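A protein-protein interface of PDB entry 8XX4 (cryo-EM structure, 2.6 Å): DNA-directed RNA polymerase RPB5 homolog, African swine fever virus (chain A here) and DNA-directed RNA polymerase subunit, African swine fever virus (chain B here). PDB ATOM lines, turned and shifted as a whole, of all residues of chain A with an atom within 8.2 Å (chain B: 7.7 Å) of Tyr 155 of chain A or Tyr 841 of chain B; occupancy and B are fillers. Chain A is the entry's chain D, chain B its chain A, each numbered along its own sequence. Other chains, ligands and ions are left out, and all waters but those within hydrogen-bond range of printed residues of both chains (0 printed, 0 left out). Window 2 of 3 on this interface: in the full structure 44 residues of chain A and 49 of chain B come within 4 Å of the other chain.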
ATOM      1  N   GLN A 148     -25.702  13.817   5.349  1.00  0.00           N
ATOM      2  CA  GLN A 148     -26.159  14.980   6.102  1.00  0.00           C
ATOM      3  C   GLN A 148     -25.423  16.239   5.679  1.00  0.00           C
ATOM      4  O   GLN A 148     -26.032  17.304   5.554  1.00  0.00           O
ATOM      5  CB  GLN A 148     -25.993  14.743   7.603  1.00  0.00           C
ATOM      6  CG  GLN A 148     -27.200  14.112   8.275  1.00  0.00           C
ATOM      7  CD  GLN A 148     -28.491  14.369   7.524  1.00  0.00           C
ATOM      8  OE1 GLN A 148     -28.982  15.496   7.475  1.00  0.00           O
ATOM      9  NE2 GLN A 148     -29.051  13.319   6.937  1.00  0.00           N
ATOM     10  N   GLU A 149     -24.113  16.145   5.456  1.00  0.00           N
ATOM     11  CA  GLU A 149     -23.392  17.337   5.025  1.00  0.00           C
ATOM     12  C   GLU A 149     -23.756  17.721   3.594  1.00  0.00           C
ATOM     13  O   GLU A 149     -23.826  18.915   3.275  1.00  0.00           O
ATOM     14  CB  GLU A 149     -21.883  17.142   5.187  1.00  0.00           C
ATOM     15  CG  GLU A 149     -21.247  16.152   4.249  1.00  0.00           C
ATOM     16  CD  GLU A 149     -20.547  16.826   3.094  1.00  0.00           C
ATOM     17  OE1 GLU A 149     -20.212  18.022   3.226  1.00  0.00           O
ATOM     18  OE2 GLU A 149     -20.331  16.164   2.055  1.00  0.00           O
ATOM     19  N   PHE A 150     -24.021  16.738   2.729  1.00  0.00           N
ATOM     20  CA  PHE A 150     -24.493  17.049   1.384  1.00  0.00           C
ATOM     21  C   PHE A 150     -25.842  17.754   1.428  1.00  0.00           C
ATOM     22  O   PHE A 150     -26.064  18.741   0.720  1.00  0.00           O
ATOM     23  CB  PHE A 150     -24.581  15.771   0.548  1.00  0.00           C
ATOM     24  CG  PHE A 150     -25.434  15.906  -0.683  1.00  0.00           C
ATOM     25  CD1 PHE A 150     -24.966  16.580  -1.793  1.00  0.00           C
ATOM     26  CD2 PHE A 150     -26.697  15.351  -0.731  1.00  0.00           C
ATOM     27  CE1 PHE A 150     -25.743  16.702  -2.922  1.00  0.00           C
ATOM     28  CE2 PHE A 150     -27.476  15.475  -1.859  1.00  0.00           C
ATOM     29  CZ  PHE A 150     -26.997  16.151  -2.953  1.00  0.00           C
ATOM     30  N   LEU A 151     -26.759  17.261   2.260  1.00  0.00           N
ATOM     31  CA  LEU A 151     -28.082  17.866   2.351  1.00  0.00           C
ATOM     32  C   LEU A 151     -28.015  19.245   2.985  1.00  0.00           C
ATOM     33  O   LEU A 151     -28.762  20.148   2.599  1.00  0.00           O
ATOM     34  CB  LEU A 151     -29.022  16.962   3.146  1.00  0.00           C
ATOM     35  CG  LEU A 151     -29.363  15.592   2.564  1.00  0.00           C
ATOM     36  CD1 LEU A 151     -30.061  14.762   3.608  1.00  0.00           C
ATOM     37  CD2 LEU A 151     -30.227  15.727   1.337  1.00  0.00           C
ATOM     38  N   GLY A 152     -27.135  19.426   3.969  1.00  0.00           N
ATOM     39  CA  GLY A 152     -26.981  20.732   4.577  1.00  0.00           C
ATOM     40  C   GLY A 152     -26.410  21.753   3.619  1.00  0.00           C
ATOM     41  O   GLY A 152     -26.826  22.914   3.618  1.00  0.00           O
ATOM     42  N   ARG A 153     -25.446  21.343   2.795  1.00  0.00           N
ATOM     43  CA  ARG A 153     -24.924  22.251   1.780  1.00  0.00           C
ATOM     44  C   ARG A 153     -25.995  22.611   0.761  1.00  0.00           C
ATOM     45  O   ARG A 153     -26.069  23.757   0.304  1.00  0.00           O
ATOM     46  CB  ARG A 153     -23.716  21.628   1.088  1.00  0.00           C
ATOM     47  CG  ARG A 153     -22.904  22.614   0.289  1.00  0.00           C
ATOM     48  CD  ARG A 153     -22.905  22.257  -1.173  1.00  0.00           C
ATOM     49  NE  ARG A 153     -22.491  23.379  -2.005  1.00  0.00           N
ATOM     50  CZ  ARG A 153     -22.978  23.630  -3.210  1.00  0.00           C
ATOM     51  NH1 ARG A 153     -23.889  22.848  -3.761  1.00  0.00           N
ATOM     52  NH2 ARG A 153     -22.534  24.687  -3.881  1.00  0.00           N
ATOM     53  N   GLU A 154     -26.834  21.648   0.393  1.00  0.00           N
ATOM     54  CA  GLU A 154     -27.863  21.842  -0.616  1.00  0.00           C
ATOM     55  C   GLU A 154     -29.178  22.351  -0.047  1.00  0.00           C
ATOM     56  O   GLU A 154     -30.112  22.583  -0.818  1.00  0.00           O
ATOM     57  CB  GLU A 154     -28.112  20.535  -1.369  1.00  0.00           C
ATOM     58  CG  GLU A 154     -26.900  19.982  -2.071  1.00  0.00           C
ATOM     59  CD  GLU A 154     -26.663  20.633  -3.408  1.00  0.00           C
ATOM     60  OE1 GLU A 154     -27.641  20.820  -4.155  1.00  0.00           O
ATOM     61  OE2 GLU A 154     -25.500  20.960  -3.713  1.00  0.00           O
ATOM     62  N   TYR A 155     -29.272  22.532   1.269  1.00  0.00           N
ATOM     63  CA  TYR A 155     -30.504  22.980   1.921  1.00  0.00           C
ATOM     64  C   TYR A 155     -31.673  22.075   1.560  1.00  0.00           C
ATOM     65  O   TYR A 155     -32.781  22.533   1.277  1.00  0.00           O
ATOM     66  CB  TYR A 155     -30.818  24.435   1.573  1.00  0.00           C
ATOM     67  CG  TYR A 155     -30.118  25.431   2.455  1.00  0.00           C
ATOM     68  CD1 TYR A 155     -30.552  25.664   3.748  1.00  0.00           C
ATOM     69  CD2 TYR A 155     -29.018  26.133   2.000  1.00  0.00           C
ATOM     70  CE1 TYR A 155     -29.911  26.571   4.557  1.00  0.00           C
ATOM     71  CE2 TYR A 155     -28.374  27.040   2.800  1.00  0.00           C
ATOM     72  CZ  TYR A 155     -28.822  27.256   4.077  1.00  0.00           C
ATOM     73  OH  TYR A 155     -28.176  28.164   4.877  1.00  0.00           O
ATOM     74  N   LEU A 156     -31.423  20.772   1.570  1.00  0.00           N
ATOM     75  CA  LEU A 156     -32.403  19.786   1.157  1.00  0.00           C
ATOM     76  C   LEU A 156     -32.799  18.915   2.337  1.00  0.00           C
ATOM     77  O   LEU A 156     -32.044  18.760   3.299  1.00  0.00           O
ATOM     78  CB  LEU A 156     -31.860  18.894   0.037  1.00  0.00           C
ATOM     79  CG  LEU A 156     -31.795  19.455  -1.379  1.00  0.00           C
ATOM     80  CD1 LEU A 156     -31.029  18.504  -2.261  1.00  0.00           C
ATOM     81  CD2 LEU A 156     -33.179  19.692  -1.930  1.00  0.00           C
ATOM     82  N   GLN A 157     -33.960  18.383   2.259  1.00  0.00           N
ATOM     83  CA  GLN A 157     -34.430  17.316   3.116  1.00  0.00           C
ATOM     84  C   GLN A 157     -34.299  15.986   2.389  1.00  0.00           C
ATOM     85  O   GLN A 157     -34.284  15.951   1.157  1.00  0.00           O
ATOM     86  CB  GLN A 157     -35.890  17.538   3.519  1.00  0.00           C
ATOM     87  CG  GLN A 157     -36.181  18.927   4.049  1.00  0.00           C
ATOM     88  CD  GLN A 157     -35.430  19.228   5.328  1.00  0.00           C
ATOM     89  OE1 GLN A 157     -34.915  20.329   5.513  1.00  0.00           O
ATOM     90  NE2 GLN A 157     -35.366  18.249   6.220  1.00  0.00           N
ATOM     91  N   PRO A 158     -34.178  14.872   3.112  1.00  0.00           N
ATOM     92  CA  PRO A 158     -34.090  13.574   2.427  1.00  0.00           C
ATOM     93  C   PRO A 158     -35.281  13.285   1.534  1.00  0.00           C
ATOM     94  O   PRO A 158     -35.139  12.575   0.532  1.00  0.00           O
ATOM     95  CB  PRO A 158     -33.995  12.579   3.588  1.00  0.00           C
ATOM     96  CG  PRO A 158     -33.403  13.360   4.692  1.00  0.00           C
ATOM     97  CD  PRO A 158     -33.936  14.748   4.558  1.00  0.00           C
ATOM     98  N   ASP A 160     -36.730  15.405  -0.358  1.00  0.00           N
ATOM     99  CA  ASP A 160     -36.597  16.185  -1.578  1.00  0.00           C
ATOM    100  C   ASP A 160     -35.727  15.509  -2.623  1.00  0.00           C
ATOM    101  O   ASP A 160     -35.739  15.935  -3.781  1.00  0.00           O
ATOM    102  CB  ASP A 160     -36.023  17.565  -1.256  1.00  0.00           C
ATOM    103  CG  ASP A 160     -36.942  18.392  -0.379  1.00  0.00           C
ATOM    104  OD1 ASP A 160     -38.043  17.911  -0.043  1.00  0.00           O
ATOM    105  OD2 ASP A 160     -36.568  19.532  -0.030  1.00  0.00           O
ATOM    106  N   VAL B 838     -35.578  25.186 -13.062  1.00  0.00           N
ATOM    107  CA  VAL B 838     -34.226  25.312 -12.530  1.00  0.00           C
ATOM    108  C   VAL B 838     -34.246  26.200 -11.294  1.00  0.00           C
ATOM    109  O   VAL B 838     -34.814  27.298 -11.311  1.00  0.00           O
ATOM    110  CB  VAL B 838     -33.281  25.872 -13.604  1.00  0.00           C
ATOM    111  CG1 VAL B 838     -31.907  26.104 -13.034  1.00  0.00           C
ATOM    112  CG2 VAL B 838     -33.200  24.931 -14.771  1.00  0.00           C
ATOM    113  N   ASP B 839     -33.631  25.731 -10.216  1.00  0.00           N
ATOM    114  CA  ASP B 839     -33.580  26.483  -8.974  1.00  0.00           C
ATOM    115  C   ASP B 839     -32.202  27.117  -8.801  1.00  0.00           C
ATOM    116  O   ASP B 839     -31.363  27.087  -9.702  1.00  0.00           O
ATOM    117  CB  ASP B 839     -33.970  25.589  -7.794  1.00  0.00           C
ATOM    118  CG  ASP B 839     -33.142  24.334  -7.703  1.00  0.00           C
ATOM    119  OD1 ASP B 839     -32.155  24.206  -8.443  1.00  0.00           O
ATOM    120  OD2 ASP B 839     -33.484  23.464  -6.881  1.00  0.00           O
ATOM    121  N   TYR B 840     -31.963  27.703  -7.627  1.00  0.00           N
ATOM    122  CA  TYR B 840     -30.749  28.480  -7.403  1.00  0.00           C
ATOM    123  C   TYR B 840     -29.495  27.625  -7.322  1.00  0.00           C
ATOM    124  O   TYR B 840     -28.388  28.167  -7.368  1.00  0.00           O
ATOM    125  CB  TYR B 840     -30.886  29.308  -6.132  1.00  0.00           C
ATOM    126  CG  TYR B 840     -31.873  30.427  -6.272  1.00  0.00           C
ATOM    127  CD1 TYR B 840     -31.735  31.368  -7.275  1.00  0.00           C
ATOM    128  CD2 TYR B 840     -32.948  30.538  -5.412  1.00  0.00           C
ATOM    129  CE1 TYR B 840     -32.635  32.389  -7.412  1.00  0.00           C
ATOM    130  CE2 TYR B 840     -33.850  31.555  -5.543  1.00  0.00           C
ATOM    131  CZ  TYR B 840     -33.690  32.476  -6.544  1.00  0.00           C
ATOM    132  OH  TYR B 840     -34.591  33.494  -6.674  1.00  0.00           O
ATOM    133  N   TYR B 841     -29.636  26.317  -7.183  1.00  0.00           N
ATOM    134  CA  TYR B 841     -28.501  25.414  -7.270  1.00  0.00           C
ATOM    135  C   TYR B 841     -28.301  24.880  -8.674  1.00  0.00           C
ATOM    136  O   TYR B 841     -27.414  24.049  -8.884  1.00  0.00           O
ATOM    137  CB  TYR B 841     -28.682  24.246  -6.305  1.00  0.00           C
ATOM    138  CG  TYR B 841     -28.503  24.608  -4.859  1.00  0.00           C
ATOM    139  CD1 TYR B 841     -29.472  25.327  -4.180  1.00  0.00           C
ATOM    140  CD2 TYR B 841     -27.376  24.214  -4.166  1.00  0.00           C
ATOM    141  CE1 TYR B 841     -29.314  25.652  -2.863  1.00  0.00           C
ATOM    142  CE2 TYR B 841     -27.214  24.527  -2.849  1.00  0.00           C
ATOM    143  CZ  TYR B 841     -28.181  25.249  -2.200  1.00  0.00           C
ATOM    144  OH  TYR B 841     -28.013  25.569  -0.877  1.00  0.00           O
ATOM    145  N   ARG B 842     -29.107  25.339  -9.626  1.00  0.00           N
ATOM    146  CA  ARG B 842     -29.166  24.864 -11.002  1.00  0.00           C
ATOM    147  C   ARG B 842     -29.628  23.421 -11.102  1.00  0.00           C
ATOM    148  O   ARG B 842     -29.491  22.802 -12.160  1.00  0.00           O
ATOM    149  CB  ARG B 842     -27.830  25.048 -11.728  1.00  0.00           C
ATOM    150  CG  ARG B 842     -27.843  26.204 -12.694  1.00  0.00           C
ATOM    151  CD  ARG B 842     -26.456  26.716 -12.972  1.00  0.00           C
ATOM    152  NE  ARG B 842     -26.476  28.138 -13.278  1.00  0.00           N
ATOM    153  CZ  ARG B 842     -25.676  29.032 -12.721  1.00  0.00           C
ATOM    154  NH1 ARG B 842     -24.761  28.682 -11.836  1.00  0.00           N
ATOM    155  NH2 ARG B 842     -25.800  30.311 -13.058  1.00  0.00           N
ATOM    156  N   ARG B 843     -30.170  22.869 -10.024  1.00  0.00           N
ATOM    157  CA  ARG B 843     -30.887  21.613 -10.101  1.00  0.00           C
ATOM    158  C   ARG B 843     -32.248  21.844 -10.736  1.00  0.00           C
ATOM    159  O   ARG B 843     -32.726  22.971 -10.852  1.00  0.00           O
ATOM    160  CB  ARG B 843     -31.069  21.002  -8.713  1.00  0.00           C
ATOM    161  CG  ARG B 843     -29.947  21.283  -7.748  1.00  0.00           C
ATOM    162  CD  ARG B 843     -30.306  20.845  -6.349  1.00  0.00           C
ATOM    163  NE  ARG B 843     -31.285  21.732  -5.737  1.00  0.00           N
ATOM    164  CZ  ARG B 843     -31.249  22.126  -4.475  1.00  0.00           C
ATOM    165  NH1 ARG B 843     -30.304  21.715  -3.651  1.00  0.00           N
ATOM    166  NH2 ARG B 843     -32.183  22.956  -4.027  1.00  0.00           N
ATOM    167  N   VAL B 844     -32.880  20.758 -11.152  1.00  0.00           N
ATOM    168  CA  VAL B 844     -34.248  20.794 -11.642  1.00  0.00           C
ATOM    169  C   VAL B 844     -35.123  20.129 -10.598  1.00  0.00           C
ATOM    170  O   VAL B 844     -34.830  19.013 -10.155  1.00  0.00           O
ATOM    171  CB  VAL B 844     -34.385  20.106 -13.008  1.00  0.00           C
ATOM    172  CG1 VAL B 844     -35.768  20.317 -13.538  1.00  0.00           C
ATOM    173  CG2 VAL B 844     -33.364  20.663 -13.970  1.00  0.00           C
ATOM    174  N   THR B 848     -40.176  21.380  -4.515  1.00  0.00           N
ATOM    175  CA  THR B 848     -38.908  21.196  -3.830  1.00  0.00           C
ATOM    176  C   THR B 848     -38.273  19.839  -4.080  1.00  0.00           C
ATOM    177  O   THR B 848     -37.106  19.653  -3.725  1.00  0.00           O
ATOM    178  CB  THR B 848     -39.083  21.384  -2.318  1.00  0.00           C
ATOM    179  OG1 THR B 848     -40.306  20.767  -1.900  1.00  0.00           O
ATOM    180  CG2 THR B 848     -39.119  22.855  -1.974  1.00  0.00           C
ATOM    181  N   LEU B 850     -36.357  17.004  -5.946  1.00  0.00           N
ATOM    182  CA  LEU B 850     -35.368  17.028  -7.012  1.00  0.00           C
ATOM    183  C   LEU B 850     -35.775  16.125  -8.164  1.00  0.00           C
ATOM    184  O   LEU B 850     -36.223  14.995  -7.963  1.00  0.00           O
ATOM    185  CB  LEU B 850     -34.004  16.595  -6.484  1.00  0.00           C
ATOM    186  CG  LEU B 850     -33.243  17.569  -5.592  1.00  0.00           C
ATOM    187  CD1 LEU B 850     -31.766  17.233  -5.625  1.00  0.00           C
ATOM    188  CD2 LEU B 850     -33.484  19.006  -6.016  1.00  0.00           C
ATOM    189  N   GLN B 852     -33.520  16.602 -11.263  1.00  0.00           N
ATOM    190  CA  GLN B 852     -32.131  16.472 -11.672  1.00  0.00           C
ATOM    191  C   GLN B 852     -31.258  17.106 -10.605  1.00  0.00           C
ATOM    192  O   GLN B 852     -31.644  18.108  -9.998  1.00  0.00           O
ATOM    193  CB  GLN B 852     -31.870  17.152 -13.014  1.00  0.00           C
ATOM    194  CG  GLN B 852     -32.779  16.707 -14.130  1.00  0.00           C
ATOM    195  CD  GLN B 852     -32.065  16.623 -15.453  1.00  0.00           C
ATOM    196  OE1 GLN B 852     -31.146  15.827 -15.620  1.00  0.00           O
ATOM    197  NE2 GLN B 852     -32.478  17.445 -16.403  1.00  0.00           N
ATOM    198  N   GLN B 853     -30.092  16.513 -10.358  1.00  0.00           N
ATOM    199  CA  GLN B 853     -29.127  17.160  -9.477  1.00  0.00           C
ATOM    200  C   GLN B 853     -28.515  18.382 -10.147  1.00  0.00           C
ATOM    201  O   GLN B 853     -28.246  19.391  -9.490  1.00  0.00           O
ATOM    202  CB  GLN B 853     -28.044  16.169  -9.065  1.00  0.00           C
ATOM    203  CG  GLN B 853     -27.035  16.743  -8.108  1.00  0.00           C
ATOM    204  CD  GLN B 853     -27.620  17.026  -6.750  1.00  0.00           C
ATOM    205  OE1 GLN B 853     -27.942  16.108  -6.003  1.00  0.00           O
ATOM    206  NE2 GLN B 853     -27.771  18.301  -6.424  1.00  0.00           N
ATOM    207  N   LEU B 854     -28.278  18.302 -11.448  1.00  0.00           N
ATOM    208  CA  LEU B 854     -27.858  19.439 -12.248  1.00  0.00           C
ATOM    209  C   LEU B 854     -28.605  19.372 -13.565  1.00  0.00           C
ATOM    210  O   LEU B 854     -28.803  18.284 -14.109  1.00  0.00           O
ATOM    211  CB  LEU B 854     -26.348  19.428 -12.488  1.00  0.00           C
ATOM    212  CG  LEU B 854     -25.691  20.733 -12.925  1.00  0.00           C
ATOM    213  CD1 LEU B 854     -26.211  21.902 -12.130  1.00  0.00           C
ATOM    214  CD2 LEU B 854     -24.211  20.613 -12.754  1.00  0.00           C
ATOM    215  N   TYR B 855     -29.030  20.523 -14.072  1.00  0.00           N
ATOM    216  CA  TYR B 855     -29.794  20.529 -15.310  1.00  0.00           C
ATOM    217  C   TYR B 855     -28.948  19.993 -16.454  1.00  0.00           C
ATOM    218  O   TYR B 855     -27.847  20.484 -16.703  1.00  0.00           O
ATOM    219  CB  TYR B 855     -30.286  21.934 -15.642  1.00  0.00           C
ATOM    220  CG  TYR B 855     -30.898  21.989 -17.015  1.00  0.00           C
ATOM    221  CD1 TYR B 855     -32.017  21.237 -17.319  1.00  0.00           C
ATOM    222  CD2 TYR B 855     -30.339  22.760 -18.020  1.00  0.00           C
ATOM    223  CE1 TYR B 855     -32.571  21.262 -18.569  1.00  0.00           C
ATOM    224  CE2 TYR B 855     -30.894  22.792 -19.276  1.00  0.00           C
ATOM    225  CZ  TYR B 855     -32.011  22.041 -19.541  1.00  0.00           C
ATOM    226  OH  TYR B 855     -32.578  22.062 -20.788  1.00  0.00           O
ATOM    227  N   GLY B 859     -25.543  21.559 -16.376  1.00  0.00           N
ATOM    228  CA  GLY B 859     -26.005  22.891 -16.025  1.00  0.00           C
ATOM    229  C   GLY B 859     -25.846  23.930 -17.109  1.00  0.00           C
ATOM    230  O   GLY B 859     -25.589  25.098 -16.801  1.00  0.00           O
ATOM    231  N   PHE B 975     -19.851  27.031 -11.344  1.00  0.00           N
ATOM    232  CA  PHE B 975     -21.172  26.624 -10.904  1.00  0.00           C
ATOM    233  C   PHE B 975     -21.542  27.190  -9.547  1.00  0.00           C
ATOM    234  O   PHE B 975     -22.673  26.985  -9.101  1.00  0.00           O
ATOM    235  CB  PHE B 975     -21.260  25.100 -10.860  1.00  0.00           C
ATOM    236  CG  PHE B 975     -21.158  24.452 -12.202  1.00  0.00           C
ATOM    237  CD1 PHE B 975     -22.191  24.551 -13.109  1.00  0.00           C
ATOM    238  CD2 PHE B 975     -20.030  23.740 -12.556  1.00  0.00           C
ATOM    239  CE1 PHE B 975     -22.098  23.957 -14.340  1.00  0.00           C
ATOM    240  CE2 PHE B 975     -19.936  23.145 -13.785  1.00  0.00           C
ATOM    241  CZ  PHE B 975     -20.971  23.256 -14.678  1.00  0.00           C
ATOM    242  N   PRO B 988     -18.857  20.324  -4.309  1.00  0.00           N
ATOM    243  CA  PRO B 988     -19.584  19.053  -4.295  1.00  0.00           C
ATOM    244  C   PRO B 988     -19.123  18.136  -5.416  1.00  0.00           C
ATOM    245  O   PRO B 988     -18.602  18.572  -6.443  1.00  0.00           O
ATOM    246  CB  PRO B 988     -21.042  19.475  -4.486  1.00  0.00           C
ATOM    247  CG  PRO B 988     -21.082  20.897  -4.119  1.00  0.00           C
ATOM    248  CD  PRO B 988     -19.760  21.471  -4.469  1.00  0.00           C
ATOM    249  N   TYR B 990     -20.852  16.261  -7.487  1.00  0.00           N
ATOM    250  CA  TYR B 990     -21.572  16.389  -8.748  1.00  0.00           C
ATOM    251  C   TYR B 990     -21.120  17.615  -9.531  1.00  0.00           C
ATOM    252  O   TYR B 990     -21.095  17.587 -10.767  1.00  0.00           O
ATOM    253  CB  TYR B 990     -23.079  16.416  -8.496  1.00  0.00           C
ATOM    254  CG  TYR B 990     -23.619  17.701  -7.917  1.00  0.00           C
ATOM    255  CD1 TYR B 990     -23.564  17.950  -6.557  1.00  0.00           C
ATOM    256  CD2 TYR B 990     -24.210  18.653  -8.730  1.00  0.00           C
ATOM    257  CE1 TYR B 990     -24.065  19.112  -6.027  1.00  0.00           C
ATOM    258  CE2 TYR B 990     -24.713  19.818  -8.207  1.00  0.00           C
ATOM    259  CZ  TYR B 990     -24.637  20.042  -6.855  1.00  0.00           C
ATOM    260  OH  TYR B 990     -25.140  21.207  -6.332  1.00  0.00           O
ATOM    261  N   LEU B 991     -20.747  18.691  -8.839  1.00  0.00           N
ATOM    262  CA  LEU B 991     -20.185  19.842  -9.529  1.00  0.00           C
ATOM    263  C   LEU B 991     -18.809  19.533 -10.099  1.00  0.00           C
ATOM    264  O   LEU B 991     -18.450  20.048 -11.162  1.00  0.00           O
ATOM    265  CB  LEU B 991     -20.119  21.036  -8.583  1.00  0.00           C
ATOM    266  CG  LEU B 991     -21.464  21.703  -8.315  1.00  0.00           C
ATOM    267  CD1 LEU B 991     -21.264  23.032  -7.634  1.00  0.00           C
ATOM    268  CD2 LEU B 991     -22.238  21.873  -9.604  1.00  0.00           C
ATOM    269  N   ILE B1035     -27.304  27.483 -17.441  1.00  0.00           N
ATOM    270  CA  ILE B1035     -28.745  27.683 -17.462  1.00  0.00           C
ATOM    271  C   ILE B1035     -29.136  28.657 -16.360  1.00  0.00           C
ATOM    272  O   ILE B1035     -28.525  28.692 -15.285  1.00  0.00           O
ATOM    273  CB  ILE B1035     -29.483  26.339 -17.326  1.00  0.00           C
ATOM    274  CG1 ILE B1035     -30.956  26.494 -17.698  1.00  0.00           C
ATOM    275  CG2 ILE B1035     -29.356  25.785 -15.925  1.00  0.00           C
ATOM    276  CD1 ILE B1035     -31.239  26.344 -19.161  1.00  0.00           C
ATOM    277  N   TYR B1037     -31.330  30.536 -13.419  1.00  0.00           N
ATOM    278  CA  TYR B1037     -32.245  30.217 -12.336  1.00  0.00           C
ATOM    279  C   TYR B1037     -33.670  30.542 -12.755  1.00  0.00           C
ATOM    280  O   TYR B1037     -33.937  31.619 -13.293  1.00  0.00           O
ATOM    281  CB  TYR B1037     -31.879  31.006 -11.083  1.00  0.00           C
ATOM    282  CG  TYR B1037     -30.450  30.845 -10.637  1.00  0.00           C
ATOM    283  CD1 TYR B1037     -29.838  29.606 -10.649  1.00  0.00           C
ATOM    284  CD2 TYR B1037     -29.716  31.933 -10.193  1.00  0.00           C
ATOM    285  CE1 TYR B1037     -28.539  29.455 -10.233  1.00  0.00           C
ATOM    286  CE2 TYR B1037     -28.414  31.791  -9.779  1.00  0.00           C
ATOM    287  CZ  TYR B1037     -27.833  30.549  -9.802  1.00  0.00           C
ATOM    288  OH  TYR B1037     -26.535  30.389  -9.391  1.00  0.00           O
ATOM    289  N   TYR B1426     -38.609  34.788 -10.934  1.00  0.00           N
ATOM    290  CA  TYR B1426     -38.122  33.754 -10.032  1.00  0.00           C
ATOM    291  C   TYR B1426     -37.475  34.363  -8.798  1.00  0.00           C
ATOM    292  O   TYR B1426     -37.758  33.943  -7.671  1.00  0.00           O
ATOM    293  CB  TYR B1426     -37.133  32.848 -10.760  1.00  0.00           C
ATOM    294  CG  TYR B1426     -36.830  31.582 -10.009  1.00  0.00           C
ATOM    295  CD1 TYR B1426     -37.813  30.635  -9.796  1.00  0.00           C
ATOM    296  CD2 TYR B1426     -35.563  31.333  -9.510  1.00  0.00           C
ATOM    297  CE1 TYR B1426     -37.548  29.482  -9.111  1.00  0.00           C
ATOM    298  CE2 TYR B1426     -35.289  30.178  -8.823  1.00  0.00           C
ATOM    299  CZ  TYR B1426     -36.286  29.257  -8.625  1.00  0.00           C
ATOM    300  OH  TYR B1426     -36.037  28.099  -7.939  1.00  0.00           O
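Of the printed residues of chain B, Glu 154 of chain A touches Tyr 841, Arg 843, Gln 853 and Tyr 990.
Tyr 155 of chain A touches one residue of chain B.
Printed residues of chain B within 4 Å of Leu 156 of chain A: Arg 843 and Leu 850.
Printed residues of chain A within 4 Å of Tyr 841 of chain B: Arg 153, Glu 154 and Tyr 155.
Printed residues of chain A within 4 Å of Leu 850 of chain B: Leu 156 (3.7 Å) and Asp 160 (2.5 Å).
Printed residues of chain A within 4 Å of Pro 988 of chain B: Arg 153.
Of the printed residues of chain A, Tyr 990 of chain B touches Arg 153 (3.3 Å) and Glu 154 (2.7 Å).
The nearest residue of chain B that does not touch Tyr 155 of chain A is Arg 843 of chain B (5.1 Å).
The side-chain carboxylate (OD2) of Asp 839 of chain B is in salt-bridge range of the guanidinium group (NE) of Arg 843 of chain B (3.0 Å).
O of Leu 151 of chain A is in hydrogen-bond range of N of Leu 156 of chain A (2.9 Å).
The side-chain carboxylate (OE2) of Glu 154 of chain A is in salt-bridge range of the guanidinium group (NH1) of Arg 153 of chain A (2.5 Å).
OH of Tyr 841 of chain B sits at hydrogen-bond distance from O of Arg 153 of chain A (2.9 Å).
OE1 of Glu 154 of chain A lies within salt-bridge range of NH1 of Arg 843 of chain B (2.9 Å).
The backbone carbonyl oxygen (O) of Asp 160 of chain A sits at hydrogen-bond distance from the backbone NH (N) of Leu 850 of chain B (2.5 Å).
The side-chain amide nitrogen (NE2) of Gln 853 of chain B is in hydrogen-bond range of the side-chain carboxylate (OE1) of Glu 154 of chain A.
NH1 of Arg 153 of chain A lies within hydrogen-bond range of OH of Tyr 990 of chain B.
OH of Tyr 990 of chain B sits at hydrogen-bond distance from OE2 of Glu 154 of chain A (2.7 Å).
Among the printed residues, merely in contact across the chains: Tyr 155 of chain A with Tyr 841 of chain B, Phe 150 of chain A with Gln 853 of chain B, Glu 154 of chain A with Tyr 841 of chain B, Asp 160 of chain A with Thr 848 of chain B, Arg 153 of chain A with Pro 988 of chain B, Leu 156 of chain A with Arg 843 of chain B and Leu 156 of chain A with Leu 850 of chain B.
Of the 12 printed residues of chain A, 6 touch a printed residue of chain B.
Hydrophobic or aromatic side chains of chain A within 4 Å of the printed part of chain B: Phe 150, Tyr 155 and Leu 156.
Of the 21 printed residues of chain B, 7 touch a printed residue of chain A.
Printed residues of chain B that touch a printed residue of chain A: Tyr 841, Arg 843, Thr 848, Leu 850, Gln 853, Pro 988 and Tyr 990.
Hydrophobic or aromatic side chains of chain B within 4 Å of the printed part of chain A: Tyr 841, Leu 850, Pro 988 and Tyr 990.
Among the printed residues, Asp or Glu carboxylates within 4 Å of a Lys or Arg side-chain nitrogen of the other chain: Glu 154 of chain A with Arg 843 of chain B (2.9 Å).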
